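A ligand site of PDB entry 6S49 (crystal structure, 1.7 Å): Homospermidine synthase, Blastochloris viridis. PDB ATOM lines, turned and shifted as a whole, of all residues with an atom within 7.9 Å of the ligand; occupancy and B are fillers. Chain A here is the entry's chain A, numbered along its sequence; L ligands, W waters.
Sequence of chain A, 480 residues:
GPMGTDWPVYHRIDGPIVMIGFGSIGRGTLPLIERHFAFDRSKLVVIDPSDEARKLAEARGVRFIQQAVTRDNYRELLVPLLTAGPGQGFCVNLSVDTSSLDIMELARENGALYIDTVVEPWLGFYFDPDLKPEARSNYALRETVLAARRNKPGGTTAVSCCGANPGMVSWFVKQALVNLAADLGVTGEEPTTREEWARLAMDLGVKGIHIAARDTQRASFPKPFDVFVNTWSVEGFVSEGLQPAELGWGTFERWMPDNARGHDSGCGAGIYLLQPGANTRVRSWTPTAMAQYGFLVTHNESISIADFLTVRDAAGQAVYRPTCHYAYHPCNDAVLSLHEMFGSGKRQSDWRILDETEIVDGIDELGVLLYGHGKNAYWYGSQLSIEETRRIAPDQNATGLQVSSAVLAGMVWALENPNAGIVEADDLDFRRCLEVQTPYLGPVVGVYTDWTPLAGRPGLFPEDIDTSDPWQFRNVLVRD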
ATOM      1  N   ARG A 142       3.019 -21.000   2.077  1.00  0.00           N
ATOM      2  CA  ARG A 142       2.753 -19.937   1.104  1.00  0.00           C
ATOM      3  C   ARG A 142       3.474 -20.218  -0.202  1.00  0.00           C
ATOM      4  O   ARG A 142       2.948 -19.926  -1.290  1.00  0.00           O
ATOM      5  CB  ARG A 142       3.165 -18.591   1.691  1.00  0.00           C
ATOM      6  CG  ARG A 142       3.022 -17.437   0.731  1.00  0.00           C
ATOM      7  CD  ARG A 142       3.309 -16.126   1.412  1.00  0.00           C
ATOM      8  NE  ARG A 142       3.183 -15.019   0.492  1.00  0.00           N
ATOM      9  CZ  ARG A 142       4.203 -14.453  -0.159  1.00  0.00           C
ATOM     10  NH1 ARG A 142       5.431 -14.891   0.034  1.00  0.00           N
ATOM     11  NH2 ARG A 142       3.988 -13.455  -0.996  1.00  0.00           N
ATOM     12  N   LEU A 146       2.403 -19.774  -4.252  1.00  0.00           N
ATOM     13  CA  LEU A 146       3.158 -19.034  -5.266  1.00  0.00           C
ATOM     14  C   LEU A 146       3.579 -19.944  -6.417  1.00  0.00           C
ATOM     15  O   LEU A 146       3.577 -19.531  -7.579  1.00  0.00           O
ATOM     16  CB  LEU A 146       4.390 -18.370  -4.631  1.00  0.00           C
ATOM     17  CG  LEU A 146       4.210 -17.436  -3.418  1.00  0.00           C
ATOM     18  CD1 LEU A 146       5.499 -16.641  -3.144  1.00  0.00           C
ATOM     19  CD2 LEU A 146       3.067 -16.488  -3.570  1.00  0.00           C
ATOM     20  N   ARG A 149       0.596 -20.473  -8.649  1.00  0.00           N
ATOM     21  CA  ARG A 149       0.371 -19.314  -9.489  1.00  0.00           C
ATOM     22  C   ARG A 149       1.328 -19.297 -10.668  1.00  0.00           C
ATOM     23  O   ARG A 149       0.917 -18.987 -11.794  1.00  0.00           O
ATOM     24  CB  ARG A 149       0.523 -18.038  -8.673  1.00  0.00           C
ATOM     25  CG  ARG A 149       0.545 -16.774  -9.519  1.00  0.00           C
ATOM     26  CD  ARG A 149       0.151 -15.565  -8.666  1.00  0.00           C
ATOM     27  NE  ARG A 149       1.168 -15.227  -7.689  1.00  0.00           N
ATOM     28  CZ  ARG A 149       0.977 -14.483  -6.611  1.00  0.00           C
ATOM     29  NH1 ARG A 149      -0.227 -14.007  -6.324  1.00  0.00           N
ATOM     30  NH2 ARG A 149       2.016 -14.226  -5.823  1.00  0.00           N
ATOM     31  N   GLY A 154      -2.870 -16.230 -14.211  1.00  0.00           N
ATOM     32  CA  GLY A 154      -4.176 -15.773 -14.616  1.00  0.00           C
ATOM     33  C   GLY A 154      -5.260 -16.799 -14.326  1.00  0.00           C
ATOM     34  O   GLY A 154      -5.133 -17.673 -13.481  1.00  0.00           O
ATOM     35  N   LYS A 174      -1.150  -0.259   3.314  1.00  0.00           N
ATOM     36  CA  LYS A 174      -1.156   0.714   2.232  1.00  0.00           C
ATOM     37  C   LYS A 174      -1.687   2.066   2.700  1.00  0.00           C
ATOM     38  O   LYS A 174      -1.082   3.109   2.403  1.00  0.00           O
ATOM     39  CB  LYS A 174      -1.956   0.174   1.045  1.00  0.00           C
ATOM     40  CG  LYS A 174      -1.211  -0.851   0.235  1.00  0.00           C
ATOM     41  CD  LYS A 174      -2.018  -1.278  -0.974  1.00  0.00           C
ATOM     42  CE  LYS A 174      -1.288  -2.258  -1.871  1.00  0.00           C
ATOM     43  NZ  LYS A 174      -1.277  -3.607  -1.272  1.00  0.00           N
ATOM     44  N   ARG A 194       2.992  -2.854  -7.472  1.00  0.00           N
ATOM     45  CA  ARG A 194       3.763  -3.415  -6.371  1.00  0.00           C
ATOM     46  C   ARG A 194       5.122  -2.728  -6.234  1.00  0.00           C
ATOM     47  O   ARG A 194       5.539  -2.367  -5.130  1.00  0.00           O
ATOM     48  CB  ARG A 194       3.942  -4.918  -6.569  1.00  0.00           C
ATOM     49  CG  ARG A 194       4.930  -5.571  -5.633  1.00  0.00           C
ATOM     50  CD  ARG A 194       5.086  -7.050  -5.880  1.00  0.00           C
ATOM     51  NE  ARG A 194       5.395  -7.339  -7.281  1.00  0.00           N
ATOM     52  CZ  ARG A 194       6.598  -7.242  -7.822  1.00  0.00           C
ATOM     53  NH1 ARG A 194       7.635  -6.861  -7.075  1.00  0.00           N
ATOM     54  NH2 ARG A 194       6.785  -7.519  -9.102  1.00  0.00           N
ATOM     55  N   CYS A 267      10.603 -16.986  -2.095  1.00  0.00           N
ATOM     56  CA  CYS A 267      10.629 -15.562  -2.362  1.00  0.00           C
ATOM     57  C   CYS A 267      11.744 -14.863  -1.598  1.00  0.00           C
ATOM     58  O   CYS A 267      12.102 -13.733  -1.950  1.00  0.00           O
ATOM     59  CB  CYS A 267       9.259 -14.942  -2.025  1.00  0.00           C
ATOM     60  SG  CYS A 267       8.922 -14.859  -0.250  1.00  0.00           S
ATOM     61  N   ILE A 303       5.076 -12.879   6.004  1.00  0.00           N
ATOM     62  CA  ILE A 303       5.845 -13.094   4.780  1.00  0.00           C
ATOM     63  C   ILE A 303       5.301 -12.257   3.637  1.00  0.00           C
ATOM     64  O   ILE A 303       6.051 -11.604   2.911  1.00  0.00           O
ATOM     65  CB  ILE A 303       5.845 -14.592   4.407  1.00  0.00           C
ATOM     66  CG1 ILE A 303       6.249 -15.463   5.601  1.00  0.00           C
ATOM     67  CG2 ILE A 303       6.802 -14.821   3.230  1.00  0.00           C
ATOM     68  CD1 ILE A 303       7.552 -15.018   6.292  1.00  0.00           C
ATOM     69  N   SER A 304       3.975 -12.241   3.433  1.00  0.00           N
ATOM     70  CA  SER A 304       3.442 -11.654   2.204  1.00  0.00           C
ATOM     71  C   SER A 304       3.679 -10.146   2.150  1.00  0.00           C
ATOM     72  O   SER A 304       4.000  -9.613   1.094  1.00  0.00           O
ATOM     73  CB  SER A 304       1.951 -11.992   2.033  1.00  0.00           C
ATOM     74  OG  SER A 304       1.087 -11.119   2.736  1.00  0.00           O
ATOM     75  N   ILE A 305       3.530  -9.457   3.284  1.00  0.00           N
ATOM     76  CA  ILE A 305       3.754  -8.016   3.289  1.00  0.00           C
ATOM     77  C   ILE A 305       5.220  -7.703   3.054  1.00  0.00           C
ATOM     78  O   ILE A 305       5.559  -6.796   2.276  1.00  0.00           O
ATOM     79  CB  ILE A 305       3.240  -7.396   4.604  1.00  0.00           C
ATOM     80  CG1 ILE A 305       1.705  -7.548   4.706  1.00  0.00           C
ATOM     81  CG2 ILE A 305       3.691  -5.939   4.701  1.00  0.00           C
ATOM     82  CD1 ILE A 305       1.104  -7.133   6.057  1.00  0.00           C
ATOM     83  N   ALA A 306       6.131  -8.428   3.717  1.00  0.00           N
ATOM     84  CA  ALA A 306       7.556  -8.186   3.497  1.00  0.00           C
ATOM     85  C   ALA A 306       7.925  -8.450   2.044  1.00  0.00           C
ATOM     86  O   ALA A 306       8.722  -7.714   1.461  1.00  0.00           O
ATOM     87  CB  ALA A 306       8.384  -9.051   4.445  1.00  0.00           C
ATOM     88  N   ASP A 307       7.375  -9.527   1.461  1.00  0.00           N
ATOM     89  CA  ASP A 307       7.616  -9.856   0.061  1.00  0.00           C
ATOM     90  C   ASP A 307       7.098  -8.758  -0.858  1.00  0.00           C
ATOM     91  O   ASP A 307       7.821  -8.272  -1.732  1.00  0.00           O
ATOM     92  CB  ASP A 307       6.948 -11.214  -0.245  1.00  0.00           C
ATOM     93  CG  ASP A 307       7.251 -11.756  -1.639  1.00  0.00           C
ATOM     94  OD1 ASP A 307       8.285 -11.381  -2.245  1.00  0.00           O
ATOM     95  OD2 ASP A 307       6.430 -12.581  -2.116  1.00  0.00           O
ATOM     96  N   PHE A 308       5.861  -8.331  -0.623  1.00  0.00           N
ATOM     97  CA  PHE A 308       5.226  -7.308  -1.457  1.00  0.00           C
ATOM     98  C   PHE A 308       6.030  -6.021  -1.467  1.00  0.00           C
ATOM     99  O   PHE A 308       6.190  -5.373  -2.509  1.00  0.00           O
ATOM    100  CB  PHE A 308       3.809  -7.058  -0.947  1.00  0.00           C
ATOM    101  CG  PHE A 308       3.037  -6.059  -1.749  1.00  0.00           C
ATOM    102  CD1 PHE A 308       2.473  -6.408  -2.960  1.00  0.00           C
ATOM    103  CD2 PHE A 308       2.878  -4.760  -1.291  1.00  0.00           C
ATOM    104  CE1 PHE A 308       1.764  -5.473  -3.696  1.00  0.00           C
ATOM    105  CE2 PHE A 308       2.177  -3.847  -2.021  1.00  0.00           C
ATOM    106  CZ  PHE A 308       1.608  -4.202  -3.226  1.00  0.00           C
ATOM    107  N   LEU A 309       6.576  -5.642  -0.311  1.00  0.00           N
ATOM    108  CA  LEU A 309       7.308  -4.396  -0.167  1.00  0.00           C
ATOM    109  C   LEU A 309       8.807  -4.566  -0.394  1.00  0.00           C
ATOM    110  O   LEU A 309       9.590  -3.718   0.052  1.00  0.00           O
ATOM    111  CB  LEU A 309       7.030  -3.802   1.214  1.00  0.00           C
ATOM    112  CG  LEU A 309       5.590  -3.361   1.466  1.00  0.00           C
ATOM    113  CD1 LEU A 309       5.429  -2.853   2.881  1.00  0.00           C
ATOM    114  CD2 LEU A 309       5.105  -2.283   0.466  1.00  0.00           C
ATOM    115  N   THR A 310       9.232  -5.617  -1.103  1.00  0.00           N
ATOM    116  CA  THR A 310      10.633  -5.842  -1.400  1.00  0.00           C
ATOM    117  C   THR A 310      11.039  -5.067  -2.654  1.00  0.00           C
ATOM    118  O   THR A 310      10.337  -5.105  -3.668  1.00  0.00           O
ATOM    119  CB  THR A 310      10.915  -7.334  -1.607  1.00  0.00           C
ATOM    120  OG1 THR A 310      10.763  -8.035  -0.364  1.00  0.00           O
ATOM    121  CG2 THR A 310      12.340  -7.584  -2.110  1.00  0.00           C
ATOM    122  N   TRP A 413     -14.507  -7.839  -4.171  1.00  0.00           N
ATOM    123  CA  TRP A 413     -13.409  -7.583  -5.103  1.00  0.00           C
ATOM    124  C   TRP A 413     -13.299  -8.699  -6.134  1.00  0.00           C
ATOM    125  O   TRP A 413     -13.082  -8.428  -7.328  1.00  0.00           O
ATOM    126  CB  TRP A 413     -12.079  -7.400  -4.352  1.00  0.00           C
ATOM    127  CG  TRP A 413     -10.970  -6.983  -5.266  1.00  0.00           C
ATOM    128  CD1 TRP A 413     -10.575  -5.702  -5.555  1.00  0.00           C
ATOM    129  CD2 TRP A 413     -10.102  -7.843  -6.018  1.00  0.00           C
ATOM    130  NE1 TRP A 413      -9.515  -5.715  -6.444  1.00  0.00           N
ATOM    131  CE2 TRP A 413      -9.230  -7.016  -6.759  1.00  0.00           C
ATOM    132  CE3 TRP A 413     -10.013  -9.237  -6.176  1.00  0.00           C
ATOM    133  CZ2 TRP A 413      -8.257  -7.539  -7.612  1.00  0.00           C
ATOM    134  CZ3 TRP A 413      -9.039  -9.744  -7.014  1.00  0.00           C
ATOM    135  CH2 TRP A 413      -8.196  -8.901  -7.738  1.00  0.00           C
ATOM    136  N   ALA A 420      -8.512 -12.660 -12.265  1.00  0.00           N
ATOM    137  CA  ALA A 420      -7.255 -12.106 -11.777  1.00  0.00           C
ATOM    138  C   ALA A 420      -6.246 -13.156 -11.341  1.00  0.00           C
ATOM    139  O   ALA A 420      -5.137 -12.800 -10.914  1.00  0.00           O
ATOM    140  CB  ALA A 420      -7.542 -11.168 -10.594  1.00  0.00           C
ATOM    141  N   GLY A 421      -6.599 -14.443 -11.414  1.00  0.00           N
ATOM    142  CA  GLY A 421      -5.704 -15.496 -10.972  1.00  0.00           C
ATOM    143  C   GLY A 421      -5.638 -15.601  -9.449  1.00  0.00           C
ATOM    144  O   GLY A 421      -6.467 -15.048  -8.710  1.00  0.00           O
ATOM    145  N   ILE A 422      -4.647 -16.362  -8.994  1.00  0.00           N
ATOM    146  CA  ILE A 422      -4.390 -16.499  -7.563  1.00  0.00           C
ATOM    147  C   ILE A 422      -3.819 -15.183  -7.047  1.00  0.00           C
ATOM    148  O   ILE A 422      -2.834 -14.672  -7.585  1.00  0.00           O
ATOM    149  CB  ILE A 422      -3.429 -17.667  -7.299  1.00  0.00           C
ATOM    150  CG1 ILE A 422      -4.101 -18.990  -7.658  1.00  0.00           C
ATOM    151  CG2 ILE A 422      -2.989 -17.674  -5.831  1.00  0.00           C
ATOM    152  CD1 ILE A 422      -3.128 -20.175  -7.810  1.00  0.00           C
ATOM    153  N   VAL A 423      -4.446 -14.624  -6.010  1.00  0.00           N
ATOM    154  CA  VAL A 423      -4.030 -13.342  -5.457  1.00  0.00           C
ATOM    155  C   VAL A 423      -4.045 -13.398  -3.934  1.00  0.00           C
ATOM    156  O   VAL A 423      -4.812 -14.134  -3.324  1.00  0.00           O
ATOM    157  CB  VAL A 423      -4.936 -12.201  -5.946  1.00  0.00           C
ATOM    158  CG1 VAL A 423      -4.687 -11.931  -7.444  1.00  0.00           C
ATOM    159  CG2 VAL A 423      -6.400 -12.520  -5.698  1.00  0.00           C
ATOM    160  N   GLU A 424      -3.186 -12.578  -3.333  1.00  0.00           N
ATOM    161  CA  GLU A 424      -3.223 -12.306  -1.906  1.00  0.00           C
ATOM    162  C   GLU A 424      -3.829 -10.941  -1.638  1.00  0.00           C
ATOM    163  O   GLU A 424      -4.065 -10.149  -2.555  1.00  0.00           O
ATOM    164  CB  GLU A 424      -1.820 -12.393  -1.296  1.00  0.00           C
ATOM    165  CG  GLU A 424      -1.248 -13.805  -1.286  1.00  0.00           C
ATOM    166  CD  GLU A 424       0.168 -13.864  -0.751  1.00  0.00           C
ATOM    167  OE1 GLU A 424       1.043 -13.153  -1.286  1.00  0.00           O
ATOM    168  OE2 GLU A 424       0.402 -14.652   0.184  1.00  0.00           O
ATOM    169  N   ALA A 425      -4.079 -10.639  -0.363  1.00  0.00           N
ATOM    170  CA  ALA A 425      -4.715  -9.374  -0.031  1.00  0.00           C
ATOM    171  C   ALA A 425      -3.850  -8.191  -0.452  1.00  0.00           C
ATOM    172  O   ALA A 425      -4.384  -7.100  -0.726  1.00  0.00           O
ATOM    173  CB  ALA A 425      -5.012  -9.315   1.475  1.00  0.00           C
ATOM    174  N   ASP A 426      -2.532  -8.377  -0.523  1.00  0.00           N
ATOM    175  CA  ASP A 426      -1.626  -7.332  -0.990  1.00  0.00           C
ATOM    176  C   ASP A 426      -1.867  -6.964  -2.453  1.00  0.00           C
ATOM    177  O   ASP A 426      -1.513  -5.856  -2.860  1.00  0.00           O
ATOM    178  CB  ASP A 426      -0.188  -7.779  -0.820  1.00  0.00           C
ATOM    179  CG  ASP A 426       0.125  -8.209   0.609  1.00  0.00           C
ATOM    180  OD1 ASP A 426       0.139  -7.336   1.488  1.00  0.00           O
ATOM    181  OD2 ASP A 426       0.273  -9.419   0.847  1.00  0.00           O
ATOM    182  N   ASP A 427      -2.449  -7.872  -3.226  1.00  0.00           N
ATOM    183  CA  ASP A 427      -2.688  -7.664  -4.646  1.00  0.00           C
ATOM    184  C   ASP A 427      -4.035  -7.015  -4.945  1.00  0.00           C
ATOM    185  O   ASP A 427      -4.279  -6.626  -6.093  1.00  0.00           O
ATOM    186  CB  ASP A 427      -2.619  -9.003  -5.378  1.00  0.00           C
ATOM    187  CG  ASP A 427      -1.306  -9.693  -5.175  1.00  0.00           C
ATOM    188  OD1 ASP A 427      -0.281  -9.004  -5.371  1.00  0.00           O
ATOM    189  OD2 ASP A 427      -1.282 -10.888  -4.799  1.00  0.00           O
ATOM    190  N   LEU A 428      -4.914  -6.889  -3.958  1.00  0.00           N
ATOM    191  CA  LEU A 428      -6.236  -6.328  -4.196  1.00  0.00           C
ATOM    192  C   LEU A 428      -6.207  -4.803  -4.139  1.00  0.00           C
ATOM    193  O   LEU A 428      -5.292  -4.197  -3.585  1.00  0.00           O
ATOM    194  CB  LEU A 428      -7.229  -6.853  -3.171  1.00  0.00           C
ATOM    195  CG  LEU A 428      -7.186  -8.341  -2.831  1.00  0.00           C
ATOM    196  CD1 LEU A 428      -8.419  -8.671  -1.988  1.00  0.00           C
ATOM    197  CD2 LEU A 428      -7.116  -9.227  -4.041  1.00  0.00           C
HETATM  198  N1  LIG L   1      -1.111 -11.061  -9.821  1.00  0.00           N
HETATM  199  C1  LIG L   1      -0.280 -11.523  -8.726  1.00  0.00           C
HETATM  200  C2  LIG L   1       0.719 -10.430  -8.341  1.00  0.00           C
HETATM  201  C3  LIG L   1       1.646 -10.905  -7.233  1.00  0.00           C
HETATM  202  C4  LIG L   1       2.589  -9.792  -6.786  1.00  0.00           C
HETATM  203  N2  LIG L   1       3.543 -10.249  -5.798  1.00  0.00           N
HETATM  204  C5  LIG L   1       3.304 -10.205  -4.489  1.00  0.00           C
HETATM  205  N3  LIG L   1       2.220  -9.756  -4.036  1.00  0.00           N
HETATM  206  N4  LIG L   1       4.237 -10.641  -3.643  1.00  0.00           N
HETATM  207  O   HOH W   1      -2.634 -13.546  -9.999  1.00  0.00           O
HETATM  208  O   HOH W   2       0.533 -10.821 -11.998  1.00  0.00           O
HETATM  209  O   HOH W   3       6.651 -10.809  -5.747  1.00  0.00           O
HETATM  210  O   HOH W   4      -2.054  -8.537  -9.181  1.00  0.00           O
HETATM  211  O   HOH W   5       0.697 -12.515  -3.871  1.00  0.00           O
HETATM  212  O   HOH W   6      -3.808 -10.550 -11.296  1.00  0.00           O
HETATM  213  O   HOH W   7       2.373 -10.472  -1.326  1.00  0.00           O
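The side-chain carboxylate of Asp 427 lies within salt-bridge range of a nitrogen (N3) of the ligand, 2.9 Å away. The side-chain carboxylate (OD2) of Asp 307 is in salt-bridge range of a nitrogen (N4) of the ligand, at 3.3 Å.
The side-chain carboxylate of Asp 427 is in salt-bridge range of the guanidinium group of Arg 149, at 3.6 Å. The side-chain carboxylate (OD2) of Asp 427 is in hydrogen-bond range of the backbone NH (N) of Glu 424 (2.9 Å). The side-chain carboxylate of Asp 307 lies within salt-bridge range of the guanidinium group of Arg 142 (2.8 Å). The backbone carbonyl oxygen (O) of Asp 307 lies close to the side-chain hydroxyl (OG1) of Thr 310, 3.3 Å away. The guanidinium group (NH1) of Arg 149 lies within hydrogen-bond range of the backbone carbonyl oxygen (O) of Ile 422, 3.0 Å away. OE2 of Glu 424 lies within salt-bridge range of NE of Arg 142 (2.8 Å). The guanidinium group (NH1) of Arg 142 sits at hydrogen-bond distance from the side-chain sulfur (SG) of Cys 267 (3.5 Å).
Arg 142 touches the ligand (NH2 to N4, 3.9 Å). Arg 149 touches the ligand (NH1 to C1, 3.5 Å). CD of Arg 194 touches N2 of the ligand, 3.6 Å away. CD1 of Phe 308 touches N3 of the ligand, 3.5 Å away. Hydrophobic or aromatic side chains within 4 Å of the ligand: Phe 308. Of the 25 residues printed, 6 come within 4 Å of the ligand.
Water W1 lies within hydrogen-bond range of O of Ile 422 (2.7 Å), O of Ala 420 (2.8 Å) and N1 of the ligand (2.9 Å). Water W6 lies within hydrogen-bond range of the backbone carbonyl oxygen (O) of Ala 420 (2.6 Å) and a nitrogen (N1) of the ligand (3.1 Å). Water W5 lies within hydrogen-bond range of the side-chain carboxylate (OE1) of Glu 424 (2.7 Å), the side-chain carboxylate (OD2) of Asp 427 (2.7 Å), the guanidinium group (NH2) of Arg 149 (2.9 Å) and a nitrogen (N3) of the ligand (3.2 Å).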
